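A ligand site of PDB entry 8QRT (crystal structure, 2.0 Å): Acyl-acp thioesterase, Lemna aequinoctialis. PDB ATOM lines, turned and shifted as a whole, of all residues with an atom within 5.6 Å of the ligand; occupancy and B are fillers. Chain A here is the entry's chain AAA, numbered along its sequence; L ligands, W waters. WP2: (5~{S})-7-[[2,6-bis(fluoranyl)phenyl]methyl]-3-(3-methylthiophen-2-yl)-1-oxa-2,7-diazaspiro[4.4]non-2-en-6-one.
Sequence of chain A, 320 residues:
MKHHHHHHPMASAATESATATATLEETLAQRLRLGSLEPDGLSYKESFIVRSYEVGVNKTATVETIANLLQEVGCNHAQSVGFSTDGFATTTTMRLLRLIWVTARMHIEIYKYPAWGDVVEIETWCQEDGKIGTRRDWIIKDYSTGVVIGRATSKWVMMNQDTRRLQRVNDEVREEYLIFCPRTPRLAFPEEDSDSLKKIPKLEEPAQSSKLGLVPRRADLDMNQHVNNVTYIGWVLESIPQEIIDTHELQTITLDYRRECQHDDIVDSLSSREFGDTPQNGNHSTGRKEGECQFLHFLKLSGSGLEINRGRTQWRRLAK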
ATOM      1  N   LEU A  70      19.786  -8.618  18.638  1.00  0.00           N
ATOM      2  CA  LEU A  70      18.989  -9.782  18.151  1.00  0.00           C
ATOM      3  C   LEU A  70      18.029  -9.310  17.044  1.00  0.00           C
ATOM      4  O   LEU A  70      17.947  -9.972  16.010  1.00  0.00           O
ATOM      5  CB  LEU A  70      18.205 -10.394  19.316  1.00  0.00           C
ATOM      6  CG  LEU A  70      19.021 -11.043  20.429  1.00  0.00           C
ATOM      7  CD1 LEU A  70      18.071 -11.584  21.488  1.00  0.00           C
ATOM      8  CD2 LEU A  70      19.920 -12.142  19.862  1.00  0.00           C
ATOM      9  N   GLN A  71      17.354  -8.174  17.264  1.00  0.00           N
ATOM     10  CA  GLN A  71      16.418  -7.562  16.274  1.00  0.00           C
ATOM     11  C   GLN A  71      17.199  -7.198  14.990  1.00  0.00           C
ATOM     12  O   GLN A  71      16.699  -7.491  13.898  1.00  0.00           O
ATOM     13  CB  GLN A  71      15.753  -6.345  16.915  1.00  0.00           C
ATOM     14  CG  GLN A  71      14.981  -5.438  15.948  1.00  0.00           C
ATOM     15  CD  GLN A  71      13.592  -5.940  15.666  1.00  0.00           C
ATOM     16  OE1 GLN A  71      13.021  -5.623  14.630  1.00  0.00           O
ATOM     17  NE2 GLN A  71      13.039  -6.720  16.593  1.00  0.00           N
ATOM     18  N   GLY A  74      18.244 -10.235  12.890  1.00  0.00           N
ATOM     19  CA  GLY A  74      16.993 -10.778  12.316  1.00  0.00           C
ATOM     20  C   GLY A  74      16.511  -9.978  11.100  1.00  0.00           C
ATOM     21  O   GLY A  74      16.077 -10.587  10.099  1.00  0.00           O
ATOM     22  N   CYS A  75      16.556  -8.651  11.197  1.00  0.00           N
ATOM     23  CA  CYS A  75      16.131  -7.722  10.120  1.00  0.00           C
ATOM     24  C   CYS A  75      17.076  -7.844   8.912  1.00  0.00           C
ATOM     25  O   CYS A  75      16.588  -8.006   7.788  1.00  0.00           O
ATOM     26  CB  CYS A  75      16.032  -6.306  10.685  1.00  0.00           C
ATOM     27  SG  CYS A  75      15.316  -5.131   9.496  1.00  0.00           S
ATOM     28  N   HIS A  77      18.806 -10.434   8.104  1.00  0.00           N
ATOM     29  CA  HIS A  77      18.535 -11.784   7.543  1.00  0.00           C
ATOM     30  C   HIS A  77      17.285 -11.718   6.641  1.00  0.00           C
ATOM     31  O   HIS A  77      17.343 -12.196   5.509  1.00  0.00           O
ATOM     32  CB  HIS A  77      18.378 -12.798   8.668  1.00  0.00           C
ATOM     33  CG  HIS A  77      18.193 -14.197   8.168  1.00  0.00           C
ATOM     34  ND1 HIS A  77      17.653 -15.178   8.958  1.00  0.00           N
ATOM     35  CD2 HIS A  77      18.470 -14.760   6.979  1.00  0.00           C
ATOM     36  CE1 HIS A  77      17.611 -16.311   8.286  1.00  0.00           C
ATOM     37  NE2 HIS A  77      18.115 -16.077   7.045  1.00  0.00           N
ATOM     38  N   ALA A  78      16.198 -11.118   7.126  1.00  0.00           N
ATOM     39  CA  ALA A  78      14.947 -10.938   6.364  1.00  0.00           C
ATOM     40  C   ALA A  78      15.273 -10.232   5.044  1.00  0.00           C
ATOM     41  O   ALA A  78      14.825 -10.677   3.985  1.00  0.00           O
ATOM     42  CB  ALA A  78      13.920 -10.152   7.156  1.00  0.00           C
ATOM     43  N   VAL A  81      17.065 -12.402   2.255  1.00  0.00           N
ATOM     44  CA  VAL A  81      16.257 -13.455   1.564  1.00  0.00           C
ATOM     45  C   VAL A  81      15.046 -12.825   0.867  1.00  0.00           C
ATOM     46  O   VAL A  81      14.217 -13.594   0.393  1.00  0.00           O
ATOM     47  CB  VAL A  81      15.816 -14.558   2.545  1.00  0.00           C
ATOM     48  CG1 VAL A  81      17.023 -15.267   3.142  1.00  0.00           C
ATOM     49  CG2 VAL A  81      14.867 -14.054   3.633  1.00  0.00           C
ATOM     50  N   PHE A  83      12.503 -10.853   2.082  1.00  0.00           N
ATOM     51  CA  PHE A  83      11.247 -10.613   2.838  1.00  0.00           C
ATOM     52  C   PHE A  83      11.181  -9.130   3.236  1.00  0.00           C
ATOM     53  O   PHE A  83      12.168  -8.432   3.062  1.00  0.00           O
ATOM     54  CB  PHE A  83      11.120 -11.586   4.007  1.00  0.00           C
ATOM     55  CG  PHE A  83      11.047 -13.035   3.580  1.00  0.00           C
ATOM     56  CD1 PHE A  83      10.677 -13.389   2.283  1.00  0.00           C
ATOM     57  CD2 PHE A  83      11.350 -14.054   4.469  1.00  0.00           C
ATOM     58  CE1 PHE A  83      10.599 -14.718   1.903  1.00  0.00           C
ATOM     59  CE2 PHE A  83      11.259 -15.384   4.087  1.00  0.00           C
ATOM     60  CZ  PHE A  83      10.886 -15.714   2.815  1.00  0.00           C
ATOM     61  N   GLY A  87       9.288  -4.909   9.713  1.00  0.00           N
ATOM     62  CA  GLY A  87       9.055  -5.519  11.035  1.00  0.00           C
ATOM     63  C   GLY A  87       8.024  -6.627  10.998  1.00  0.00           C
ATOM     64  O   GLY A  87       7.784  -7.205  12.078  1.00  0.00           O
ATOM     65  N   PHE A  88       7.419  -6.934   9.828  1.00  0.00           N
ATOM     66  CA  PHE A  88       6.407  -8.025   9.684  1.00  0.00           C
ATOM     67  C   PHE A  88       6.980  -9.205   8.906  1.00  0.00           C
ATOM     68  O   PHE A  88       6.310 -10.257   8.831  1.00  0.00           O
ATOM     69  CB  PHE A  88       5.134  -7.477   9.022  1.00  0.00           C
ATOM     70  CG  PHE A  88       4.544  -6.311   9.764  1.00  0.00           C
ATOM     71  CD1 PHE A  88       4.166  -6.439  11.094  1.00  0.00           C
ATOM     72  CD2 PHE A  88       4.397  -5.074   9.148  1.00  0.00           C
ATOM     73  CE1 PHE A  88       3.608  -5.377  11.785  1.00  0.00           C
ATOM     74  CE2 PHE A  88       3.859  -4.008   9.853  1.00  0.00           C
ATOM     75  CZ  PHE A  88       3.468  -4.162  11.166  1.00  0.00           C
ATOM     76  N   ALA A  89       8.171  -9.043   8.326  1.00  0.00           N
ATOM     77  CA  ALA A  89       8.953 -10.074   7.606  1.00  0.00           C
ATOM     78  C   ALA A  89       8.048 -10.884   6.661  1.00  0.00           C
ATOM     79  O   ALA A  89       8.035 -12.124   6.731  1.00  0.00           O
ATOM     80  CB  ALA A  89       9.634 -10.938   8.634  1.00  0.00           C
ATOM     81  N   TRP A 101       3.610 -11.333  10.353  1.00  0.00           N
ATOM     82  CA  TRP A 101       4.134 -12.083  11.513  1.00  0.00           C
ATOM     83  C   TRP A 101       4.029 -11.175  12.726  1.00  0.00           C
ATOM     84  O   TRP A 101       4.450 -10.029  12.620  1.00  0.00           O
ATOM     85  CB  TRP A 101       5.585 -12.512  11.293  1.00  0.00           C
ATOM     86  CG  TRP A 101       5.744 -13.603  10.283  1.00  0.00           C
ATOM     87  CD1 TRP A 101       6.337 -13.496   9.065  1.00  0.00           C
ATOM     88  CD2 TRP A 101       5.278 -14.953  10.390  1.00  0.00           C
ATOM     89  NE1 TRP A 101       6.278 -14.691   8.408  1.00  0.00           N
ATOM     90  CE2 TRP A 101       5.634 -15.605   9.181  1.00  0.00           C
ATOM     91  CE3 TRP A 101       4.565 -15.671  11.354  1.00  0.00           C
ATOM     92  CZ2 TRP A 101       5.349 -16.947   8.939  1.00  0.00           C
ATOM     93  CZ3 TRP A 101       4.307 -17.002  11.128  1.00  0.00           C
ATOM     94  CH2 TRP A 101       4.689 -17.631   9.948  1.00  0.00           C
ATOM     95  N   CYS A 126      15.579 -19.382  11.097  1.00  0.00           N
ATOM     96  CA  CYS A 126      14.159 -19.673  11.364  1.00  0.00           C
ATOM     97  C   CYS A 126      13.849 -21.137  11.082  1.00  0.00           C
ATOM     98  O   CYS A 126      14.584 -21.793  10.307  1.00  0.00           O
ATOM     99  CB  CYS A 126      13.257 -18.821  10.473  1.00  0.00           C
ATOM    100  SG  CYS A 126      13.355 -17.072  10.888  1.00  0.00           S
ATOM    101  N   THR A 134       6.146 -19.798  13.133  1.00  0.00           N
ATOM    102  CA  THR A 134       7.603 -19.917  12.891  1.00  0.00           C
ATOM    103  C   THR A 134       8.343 -19.616  14.188  1.00  0.00           C
ATOM    104  O   THR A 134       7.758 -18.990  15.077  1.00  0.00           O
ATOM    105  CB  THR A 134       8.062 -19.021  11.732  1.00  0.00           C
ATOM    106  OG1 THR A 134       7.550 -17.699  11.909  1.00  0.00           O
ATOM    107  CG2 THR A 134       7.632 -19.545  10.379  1.00  0.00           C
ATOM    108  N   ARG A 135       9.573 -20.131  14.275  1.00  0.00           N
ATOM    109  CA  ARG A 135      10.550 -19.908  15.354  1.00  0.00           C
ATOM    110  C   ARG A 135      11.722 -19.145  14.742  1.00  0.00           C
ATOM    111  O   ARG A 135      12.151 -19.531  13.611  1.00  0.00           O
ATOM    112  CB  ARG A 135      10.996 -21.275  15.892  1.00  0.00           C
ATOM    113  CG  ARG A 135      11.220 -21.335  17.379  1.00  0.00           C
ATOM    114  CD  ARG A 135      11.677 -22.707  17.814  1.00  0.00           C
ATOM    115  NE  ARG A 135      13.049 -22.920  17.366  1.00  0.00           N
ATOM    116  CZ  ARG A 135      13.450 -23.851  16.501  1.00  0.00           C
ATOM    117  NH1 ARG A 135      12.568 -24.696  15.973  1.00  0.00           N
ATOM    118  NH2 ARG A 135      14.724 -23.933  16.174  1.00  0.00           N
ATOM    119  N   ARG A 136      12.213 -18.097  15.405  1.00  0.00           N
ATOM    120  CA  ARG A 136      13.563 -17.571  15.089  1.00  0.00           C
ATOM    121  C   ARG A 136      14.457 -17.862  16.292  1.00  0.00           C
ATOM    122  O   ARG A 136      14.048 -17.557  17.427  1.00  0.00           O
ATOM    123  CB  ARG A 136      13.569 -16.077  14.725  1.00  0.00           C
ATOM    124  CG  ARG A 136      14.972 -15.521  14.505  1.00  0.00           C
ATOM    125  CD  ARG A 136      15.002 -14.100  13.982  1.00  0.00           C
ATOM    126  NE  ARG A 136      14.569 -14.018  12.579  1.00  0.00           N
ATOM    127  CZ  ARG A 136      15.304 -14.343  11.518  1.00  0.00           C
ATOM    128  NH1 ARG A 136      16.530 -14.825  11.652  1.00  0.00           N
ATOM    129  NH2 ARG A 136      14.802 -14.180  10.301  1.00  0.00           N
ATOM    130  N   TRP A 138      18.622 -17.646  17.878  1.00  0.00           N
ATOM    131  CA  TRP A 138      19.933 -16.943  17.804  1.00  0.00           C
ATOM    132  C   TRP A 138      20.940 -17.633  18.723  1.00  0.00           C
ATOM    133  O   TRP A 138      20.533 -18.069  19.837  1.00  0.00           O
ATOM    134  CB  TRP A 138      19.797 -15.494  18.249  1.00  0.00           C
ATOM    135  CG  TRP A 138      18.861 -14.569  17.545  1.00  0.00           C
ATOM    136  CD1 TRP A 138      19.214 -13.542  16.703  1.00  0.00           C
ATOM    137  CD2 TRP A 138      17.447 -14.392  17.795  1.00  0.00           C
ATOM    138  NE1 TRP A 138      18.121 -12.802  16.363  1.00  0.00           N
ATOM    139  CE2 TRP A 138      17.026 -13.290  17.015  1.00  0.00           C
ATOM    140  CE3 TRP A 138      16.495 -15.073  18.544  1.00  0.00           C
ATOM    141  CZ2 TRP A 138      15.695 -12.855  16.991  1.00  0.00           C
ATOM    142  CZ3 TRP A 138      15.184 -14.635  18.534  1.00  0.00           C
ATOM    143  CH2 TRP A 138      14.792 -13.560  17.751  1.00  0.00           C
ATOM    144  N   SER A 154      12.312 -17.225  19.686  1.00  0.00           N
ATOM    145  CA  SER A 154      11.092 -16.419  19.532  1.00  0.00           C
ATOM    146  C   SER A 154      10.057 -17.267  18.780  1.00  0.00           C
ATOM    147  O   SER A 154      10.477 -18.033  17.892  1.00  0.00           O
ATOM    148  CB  SER A 154      11.415 -15.154  18.853  1.00  0.00           C
ATOM    149  OG  SER A 154      12.083 -15.429  17.630  1.00  0.00           O
ATOM    150  N   TRP A 156       6.575 -16.782  16.500  1.00  0.00           N
ATOM    151  CA  TRP A 156       5.794 -15.841  15.674  1.00  0.00           C
ATOM    152  C   TRP A 156       4.556 -16.565  15.164  1.00  0.00           C
ATOM    153  O   TRP A 156       4.649 -17.751  14.804  1.00  0.00           O
ATOM    154  CB  TRP A 156       6.640 -15.296  14.521  1.00  0.00           C
ATOM    155  CG  TRP A 156       7.915 -14.690  15.010  1.00  0.00           C
ATOM    156  CD1 TRP A 156       9.027 -15.349  15.442  1.00  0.00           C
ATOM    157  CD2 TRP A 156       8.159 -13.302  15.236  1.00  0.00           C
ATOM    158  NE1 TRP A 156       9.967 -14.465  15.893  1.00  0.00           N
ATOM    159  CE2 TRP A 156       9.467 -13.199  15.770  1.00  0.00           C
ATOM    160  CE3 TRP A 156       7.446 -12.125  14.976  1.00  0.00           C
ATOM    161  CZ2 TRP A 156      10.068 -11.982  16.040  1.00  0.00           C
ATOM    162  CZ3 TRP A 156       8.039 -10.917  15.253  1.00  0.00           C
ATOM    163  CH2 TRP A 156       9.342 -10.843  15.759  1.00  0.00           C
ATOM    164  N   TYR A 177       8.739 -19.507   2.718  1.00  0.00           N
ATOM    165  CA  TYR A 177       9.769 -19.271   3.775  1.00  0.00           C
ATOM    166  C   TYR A 177      10.581 -20.548   4.035  1.00  0.00           C
ATOM    167  O   TYR A 177      11.766 -20.400   4.327  1.00  0.00           O
ATOM    168  CB  TYR A 177       9.185 -18.641   5.036  1.00  0.00           C
ATOM    169  CG  TYR A 177       8.158 -19.445   5.811  1.00  0.00           C
ATOM    170  CD1 TYR A 177       8.510 -20.496   6.646  1.00  0.00           C
ATOM    171  CD2 TYR A 177       6.829 -19.080   5.772  1.00  0.00           C
ATOM    172  CE1 TYR A 177       7.555 -21.191   7.360  1.00  0.00           C
ATOM    173  CE2 TYR A 177       5.866 -19.755   6.490  1.00  0.00           C
ATOM    174  CZ  TYR A 177       6.228 -20.819   7.292  1.00  0.00           C
ATOM    175  OH  TYR A 177       5.261 -21.497   7.989  1.00  0.00           O
ATOM    176  N   PHE A 180      14.100 -21.082   2.996  1.00  0.00           N
ATOM    177  CA  PHE A 180      15.156 -20.277   3.680  1.00  0.00           C
ATOM    178  C   PHE A 180      15.433 -20.834   5.092  1.00  0.00           C
ATOM    179  O   PHE A 180      16.167 -20.164   5.842  1.00  0.00           O
ATOM    180  CB  PHE A 180      14.764 -18.793   3.628  1.00  0.00           C
ATOM    181  CG  PHE A 180      14.706 -18.254   2.216  1.00  0.00           C
ATOM    182  CD1 PHE A 180      15.869 -18.186   1.436  1.00  0.00           C
ATOM    183  CD2 PHE A 180      13.514 -17.850   1.655  1.00  0.00           C
ATOM    184  CE1 PHE A 180      15.813 -17.701   0.136  1.00  0.00           C
ATOM    185  CE2 PHE A 180      13.457 -17.368   0.365  1.00  0.00           C
ATOM    186  CZ  PHE A 180      14.603 -17.290  -0.394  1.00  0.00           C
ATOM    187  N   CYS A 181      14.886 -22.004   5.426  1.00  0.00           N
ATOM    188  CA  CYS A 181      14.993 -22.642   6.770  1.00  0.00           C
ATOM    189  C   CYS A 181      15.735 -23.962   6.630  1.00  0.00           C
ATOM    190  O   CYS A 181      15.501 -24.702   5.674  1.00  0.00           O
ATOM    191  CB  CYS A 181      13.646 -22.912   7.401  1.00  0.00           C
ATOM    192  SG  CYS A 181      12.676 -21.416   7.740  1.00  0.00           S
HETATM  193  C1  WP2 L   1      13.377 -10.860  14.288  1.00  0.00           C
HETATM  194  C2  WP2 L   1      12.176 -10.138  13.766  1.00  0.00           C
HETATM  195  C4  WP2 L   1      10.945  -8.271  13.365  1.00  0.00           C
HETATM  196  C7  WP2 L   1      11.007 -12.154  12.849  1.00  0.00           C
HETATM  197  C10 WP2 L   1      10.488 -14.134  11.654  1.00  0.00           C
HETATM  198  C11 WP2 L   1       9.476 -15.267  11.500  1.00  0.00           C
HETATM  199  C12 WP2 L   1       9.439 -15.485   9.972  1.00  0.00           C
HETATM  200  N13 WP2 L   1      10.612 -14.784   9.408  1.00  0.00           N
HETATM  201  C14 WP2 L   1      10.984 -14.853   7.991  1.00  0.00           C
HETATM  202  C16 WP2 L   1      12.152 -17.009   7.536  1.00  0.00           C
HETATM  203  C20 WP2 L   1      14.565 -15.724   7.070  1.00  0.00           C
HETATM  204  C21 WP2 L   1      13.438 -15.019   7.409  1.00  0.00           C
HETATM  205  C23 WP2 L   1      11.207 -14.003  10.332  1.00  0.00           C
HETATM  206  C3  WP2 L   1      12.065  -8.771  13.865  1.00  0.00           C
HETATM  207  S5  WP2 L   1       9.923  -9.526  12.656  1.00  0.00           S
HETATM  208  C6  WP2 L   1      11.141 -10.740  13.110  1.00  0.00           C
HETATM  209  N8  WP2 L   1      11.819 -13.098  13.204  1.00  0.00           N
HETATM  210  O9  WP2 L   1      11.342 -14.371  12.771  1.00  0.00           O
HETATM  211  C15 WP2 L   1      12.218 -15.646   7.634  1.00  0.00           C
HETATM  212  F17 WP2 L   1      10.954 -17.627   7.756  1.00  0.00           F
HETATM  213  C18 WP2 L   1      13.265 -17.727   7.193  1.00  0.00           C
HETATM  214  C19 WP2 L   1      14.459 -17.096   6.945  1.00  0.00           C
HETATM  215  F22 WP2 L   1      13.526 -13.705   7.498  1.00  0.00           F
HETATM  216  O24 WP2 L   1      12.198 -13.323  10.113  1.00  0.00           O
HETATM  217  C25 WP2 L   1       9.853 -12.810  12.106  1.00  0.00           C
HETATM  218  O   HOH W   1      13.336 -10.798  10.533  1.00  0.00           O
HETATM  219  O   HOH W   2      12.649  -8.096  10.360  1.00  0.00           O
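An oxygen (O24) of the ligand sits at hydrogen-bond distance from the guanidinium group (NH2) of Arg 136 (2.7 Å). NE1 of Trp 156 sits at hydrogen-bond distance from O9 of the ligand (3.4 Å).
The guanidinium group (NH2) of Arg 136 sits at hydrogen-bond distance from the side-chain sulfur (SG) of Cys 126 (3.3 Å). The side-chain sulfur of Cys 181 sits at hydrogen-bond distance from the backbone carbonyl oxygen of Cys 126. The guanidinium group (NH1) of Arg 136 is in hydrogen-bond range of a ring nitrogen (ND1) of His 77. O of Arg 136 sits at hydrogen-bond distance from N of Ser 154. O of Ala 78 lies within hydrogen-bond range of N of Phe 83, 3.0 Å away. O of Tyr 177 sits at hydrogen-bond distance from SG of Cys 181. O of Thr 134 is in hydrogen-bond range of N of Trp 156, at 2.9 Å. N of Trp 101 lies close to O of Phe 88.
O of Gly 87 lies close to S5 of the ligand, 3.2 Å away. Residues that only touch the ligand: Gln 71 (3.4 Å), His 77 (3.3 Å), Ala 78 (3.3 Å), Val 81 (3.8 Å), Phe 83 (3.6 Å), Ala 89 (3.8 Å), Trp 101 (3.6 Å), Cys 126 (3.5 Å), Thr 134 (3.1 Å), Tyr 177 (3.4 Å), Phe 180 (3.7 Å) and Cys 181 (3.8 Å). Of the 22 residues printed, 15 come within 4 Å of the ligand. The nearest printed residue that does not touch the ligand is Trp 138 (4.1 Å).
Water W1 bridges the backbone carbonyl oxygen of Gly 74 (2.8 Å) and an oxygen (O24) of the ligand (2.8 Å).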
